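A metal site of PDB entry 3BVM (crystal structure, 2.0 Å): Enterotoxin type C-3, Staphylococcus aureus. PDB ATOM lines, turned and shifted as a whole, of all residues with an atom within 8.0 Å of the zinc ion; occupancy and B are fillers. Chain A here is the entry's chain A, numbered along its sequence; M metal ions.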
ATOM      1  N   ALA A  35      25.391 -18.660  37.033  1.00  0.00           N
ATOM      2  CA  ALA A  35      24.378 -17.611  37.146  1.00  0.00           C
ATOM      3  C   ALA A  35      23.377 -17.825  36.034  1.00  0.00           C
ATOM      4  O   ALA A  35      23.722 -18.421  35.002  1.00  0.00           O
ATOM      5  CB  ALA A  35      25.022 -16.240  37.063  1.00  0.00           C
ATOM      6  N   THR A  36      22.123 -17.440  36.253  1.00  0.00           N
ATOM      7  CA  THR A  36      21.076 -17.628  35.234  1.00  0.00           C
ATOM      8  C   THR A  36      20.291 -16.344  35.081  1.00  0.00           C
ATOM      9  O   THR A  36      20.131 -15.616  36.054  1.00  0.00           O
ATOM     10  CB  THR A  36      20.109 -18.814  35.582  1.00  0.00           C
ATOM     11  OG1 THR A  36      19.713 -18.707  36.935  1.00  0.00           O
ATOM     12  CG2 THR A  36      20.800 -20.217  35.370  1.00  0.00           C
ATOM     13  N   LYS A  37      19.875 -16.047  33.837  1.00  0.00           N
ATOM     14  CA  LYS A  37      19.098 -14.860  33.547  1.00  0.00           C
ATOM     15  C   LYS A  37      19.774 -13.576  34.070  1.00  0.00           C
ATOM     16  O   LYS A  37      19.160 -12.719  34.696  1.00  0.00           O
ATOM     17  CB  LYS A  37      17.651 -15.039  34.040  1.00  0.00           C
ATOM     18  CG  LYS A  37      17.088 -16.387  33.487  1.00  0.00           C
ATOM     19  CD  LYS A  37      15.711 -16.744  34.017  1.00  0.00           C
ATOM     20  CE  LYS A  37      14.674 -15.640  33.663  1.00  0.00           C
ATOM     21  NZ  LYS A  37      13.317 -15.953  34.301  1.00  0.00           N
ATOM     22  N   VAL A  38      21.062 -13.431  33.771  1.00  0.00           N
ATOM     23  CA  VAL A  38      21.786 -12.232  34.163  1.00  0.00           C
ATOM     24  C   VAL A  38      22.137 -11.375  32.969  1.00  0.00           C
ATOM     25  O   VAL A  38      22.395 -11.877  31.868  1.00  0.00           O
ATOM     26  CB  VAL A  38      23.095 -12.547  35.048  1.00  0.00           C
ATOM     27  CG1 VAL A  38      22.681 -13.013  36.499  1.00  0.00           C
ATOM     28  CG2 VAL A  38      24.030 -13.536  34.348  1.00  0.00           C
ATOM     29  N   VAL A  81      20.244 -11.250  27.892  1.00  0.00           N
ATOM     30  CA  VAL A  81      19.919 -12.065  29.063  1.00  0.00           C
ATOM     31  C   VAL A  81      20.503 -13.447  28.816  1.00  0.00           C
ATOM     32  O   VAL A  81      20.070 -14.136  27.890  1.00  0.00           O
ATOM     33  CB  VAL A  81      18.393 -12.179  29.323  1.00  0.00           C
ATOM     34  CG1 VAL A  81      18.133 -13.069  30.580  1.00  0.00           C
ATOM     35  CG2 VAL A  81      17.756 -10.742  29.501  1.00  0.00           C
ATOM     36  N   VAL A  82      21.415 -13.862  29.702  1.00  0.00           N
ATOM     37  CA  VAL A  82      22.363 -14.946  29.531  1.00  0.00           C
ATOM     38  C   VAL A  82      22.449 -15.860  30.783  1.00  0.00           C
ATOM     39  O   VAL A  82      22.184 -15.437  31.903  1.00  0.00           O
ATOM     40  CB  VAL A  82      23.875 -14.395  29.053  1.00  0.00           C
ATOM     41  CG1 VAL A  82      23.887 -13.525  27.744  1.00  0.00           C
ATOM     42  CG2 VAL A  82      24.598 -13.636  30.076  1.00  0.00           C
ATOM     43  N   ASP A  83      22.802 -17.115  30.586  1.00  0.00           N
ATOM     44  CA  ASP A  83      23.304 -17.949  31.671  1.00  0.00           C
ATOM     45  C   ASP A  83      24.861 -18.013  31.582  1.00  0.00           C
ATOM     46  O   ASP A  83      25.436 -17.916  30.479  1.00  0.00           O
ATOM     47  CB  ASP A  83      22.625 -19.289  31.572  1.00  0.00           C
ATOM     48  CG  ASP A  83      21.121 -19.107  31.439  1.00  0.00           C
ATOM     49  OD1 ASP A  83      20.565 -18.235  32.181  1.00  0.00           O
ATOM     50  OD2 ASP A  83      20.510 -19.745  30.558  1.00  0.00           O
ATOM     51  N   VAL A  84      25.515 -18.040  32.737  1.00  0.00           N
ATOM     52  CA  VAL A  84      26.961 -18.118  32.778  1.00  0.00           C
ATOM     53  C   VAL A  84      27.304 -19.479  33.389  1.00  0.00           C
ATOM     54  O   VAL A  84      26.624 -19.955  34.310  1.00  0.00           O
ATOM     55  CB  VAL A  84      27.566 -16.905  33.527  1.00  0.00           C
ATOM     56  CG1 VAL A  84      29.052 -16.975  33.552  1.00  0.00           C
ATOM     57  CG2 VAL A  84      27.165 -15.586  32.824  1.00  0.00           C
ATOM     58  N   THR A 114      26.146 -18.178  27.291  1.00  0.00           N
ATOM     59  CA  THR A 114      25.080 -18.608  26.359  1.00  0.00           C
ATOM     60  C   THR A 114      23.756 -17.812  26.622  1.00  0.00           C
ATOM     61  O   THR A 114      23.391 -17.560  27.760  1.00  0.00           O
ATOM     62  CB  THR A 114      24.772 -20.131  26.396  1.00  0.00           C
ATOM     63  OG1 THR A 114      24.349 -20.516  27.695  1.00  0.00           O
ATOM     64  CG2 THR A 114      26.002 -21.065  25.846  1.00  0.00           C
ATOM     65  N   LYS A 115      23.044 -17.402  25.561  1.00  0.00           N
ATOM     66  CA  LYS A 115      21.814 -16.637  25.713  1.00  0.00           C
ATOM     67  C   LYS A 115      20.767 -17.565  26.377  1.00  0.00           C
ATOM     68  O   LYS A 115      20.786 -18.803  26.225  1.00  0.00           O
ATOM     69  CB  LYS A 115      21.294 -16.108  24.387  1.00  0.00           C
ATOM     70  CG  LYS A 115      22.159 -15.111  23.682  1.00  0.00           C
ATOM     71  CD  LYS A 115      21.931 -15.284  22.136  1.00  0.00           C
ATOM     72  CE  LYS A 115      22.180 -14.009  21.310  1.00  0.00           C
ATOM     73  NZ  LYS A 115      22.192 -14.418  19.826  1.00  0.00           N
ATOM     74  N   HIS A 116      19.904 -16.945  27.159  1.00  0.00           N
ATOM     75  CA  HIS A 116      18.934 -17.695  27.943  1.00  0.00           C
ATOM     76  C   HIS A 116      17.680 -18.054  27.166  1.00  0.00           C
ATOM     77  O   HIS A 116      17.216 -19.225  27.209  1.00  0.00           O
ATOM     78  CB  HIS A 116      18.613 -16.938  29.235  1.00  0.00           C
ATOM     79  CG  HIS A 116      17.302 -17.324  29.817  1.00  0.00           C
ATOM     80  ND1 HIS A 116      17.117 -18.485  30.546  1.00  0.00           N
ATOM     81  CD2 HIS A 116      16.087 -16.736  29.738  1.00  0.00           C
ATOM     82  CE1 HIS A 116      15.846 -18.596  30.889  1.00  0.00           C
ATOM     83  NE2 HIS A 116      15.214 -17.521  30.453  1.00  0.00           N
ATOM     84  N   GLU A 117      17.131 -17.041  26.466  1.00  0.00           N
ATOM     85  CA  GLU A 117      15.886 -17.180  25.649  1.00  0.00           C
ATOM     86  C   GLU A 117      16.132 -18.259  24.633  1.00  0.00           C
ATOM     87  O   GLU A 117      17.028 -18.115  23.789  1.00  0.00           O
ATOM     88  CB  GLU A 117      15.479 -15.821  24.989  1.00  0.00           C
ATOM     89  CG  GLU A 117      14.331 -15.860  23.902  1.00  0.00           C
ATOM     90  CD  GLU A 117      14.144 -14.547  23.094  1.00  0.00           C
ATOM     91  OE1 GLU A 117      13.202 -14.531  22.278  1.00  0.00           O
ATOM     92  OE2 GLU A 117      14.912 -13.524  23.243  1.00  0.00           O
ATOM     93  N   GLY A 118      15.374 -19.347  24.743  1.00  0.00           N
ATOM     94  CA  GLY A 118      15.310 -20.346  23.692  1.00  0.00           C
ATOM     95  C   GLY A 118      16.266 -21.518  23.825  1.00  0.00           C
ATOM     96  O   GLY A 118      16.351 -22.366  22.900  1.00  0.00           O
ATOM     97  N   ASN A 119      16.964 -21.591  24.955  1.00  0.00           N
ATOM     98  CA  ASN A 119      18.115 -22.461  25.067  1.00  0.00           C
ATOM     99  C   ASN A 119      17.946 -23.616  25.982  1.00  0.00           C
ATOM    100  O   ASN A 119      18.922 -24.200  26.370  1.00  0.00           O
ATOM    101  CB  ASN A 119      19.391 -21.688  25.474  1.00  0.00           C
ATOM    102  CG  ASN A 119      20.653 -22.457  25.084  1.00  0.00           C
ATOM    103  OD1 ASN A 119      20.691 -23.062  24.043  1.00  0.00           O
ATOM    104  ND2 ASN A 119      21.640 -22.484  25.969  1.00  0.00           N
ATOM    105  N   HIS A 120      16.707 -23.949  26.296  1.00  0.00           N
ATOM    106  CA  HIS A 120      16.388 -24.979  27.241  1.00  0.00           C
ATOM    107  C   HIS A 120      15.452 -26.058  26.688  1.00  0.00           C
ATOM    108  O   HIS A 120      14.624 -25.813  25.780  1.00  0.00           O
ATOM    109  CB  HIS A 120      15.834 -24.345  28.514  1.00  0.00           C
ATOM    110  CG  HIS A 120      16.852 -23.539  29.246  1.00  0.00           C
ATOM    111  ND1 HIS A 120      17.973 -24.120  29.814  1.00  0.00           N
ATOM    112  CD2 HIS A 120      16.949 -22.211  29.488  1.00  0.00           C
ATOM    113  CE1 HIS A 120      18.707 -23.185  30.391  1.00  0.00           C
ATOM    114  NE2 HIS A 120      18.108 -22.015  30.205  1.00  0.00           N
ATOM    115  N   ASP A 148      21.177 -28.516  31.094  1.00  0.00           N
ATOM    116  CA  ASP A 148      19.863 -28.190  30.726  1.00  0.00           C
ATOM    117  C   ASP A 148      19.782 -27.254  29.557  1.00  0.00           C
ATOM    118  O   ASP A 148      18.728 -26.718  29.267  1.00  0.00           O
ATOM    119  CB  ASP A 148      19.133 -27.645  31.956  1.00  0.00           C
ATOM    120  CG  ASP A 148      19.640 -26.316  32.435  1.00  0.00           C
ATOM    121  OD1 ASP A 148      20.543 -25.650  31.866  1.00  0.00           O
ATOM    122  OD2 ASP A 148      19.073 -25.947  33.472  1.00  0.00           O
ATOM    123  N   LYS A 149      20.935 -27.026  28.918  1.00  0.00           N
ATOM    124  CA  LYS A 149      21.085 -26.123  27.832  1.00  0.00           C
ATOM    125  C   LYS A 149      21.168 -26.935  26.605  1.00  0.00           C
ATOM    126  O   LYS A 149      21.831 -28.000  26.576  1.00  0.00           O
ATOM    127  CB  LYS A 149      22.371 -25.299  27.985  1.00  0.00           C
ATOM    128  CG  LYS A 149      22.412 -24.412  29.278  1.00  0.00           C
ATOM    129  CD  LYS A 149      23.758 -23.727  29.438  1.00  0.00           C
ATOM    130  CE  LYS A 149      23.739 -22.820  30.699  1.00  0.00           C
ATOM    131  NZ  LYS A 149      24.064 -23.745  31.858  1.00  0.00           N
HETATM  132 ZN    ZN M   1      18.547 -20.181  31.129  1.00  0.00          ZN
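The side-chain carboxylate (OD1) of Asp 83 sits at hydrogen-bond distance from the backbone NH (N) of Lys 37 (2.8 Å).
The backbone NH (N) of Asp 83 is in hydrogen-bond range of the backbone carbonyl oxygen (O) of Thr 114.
ND1 of His 120 is in hydrogen-bond range of O of Asp 148 (2.8 Å).
The backbone carbonyl oxygen (O) of Val 81 is in hydrogen-bond range of the backbone NH (N) of His 116, at 2.9 Å.
Of the 17 residues printed, 3 come within 4 Å of the zinc ion.
The nearest printed residue that does not touch the zinc ion is Lys 37 (4.7 Å).
The zinc ion is bound by the side-chain carboxylate (OD2) of Asp 83 (2.1 Å), a ring nitrogen (NE2) of His 120 (2.1 Å) and a ring nitrogen (ND1) of His 116 (2.3 Å).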
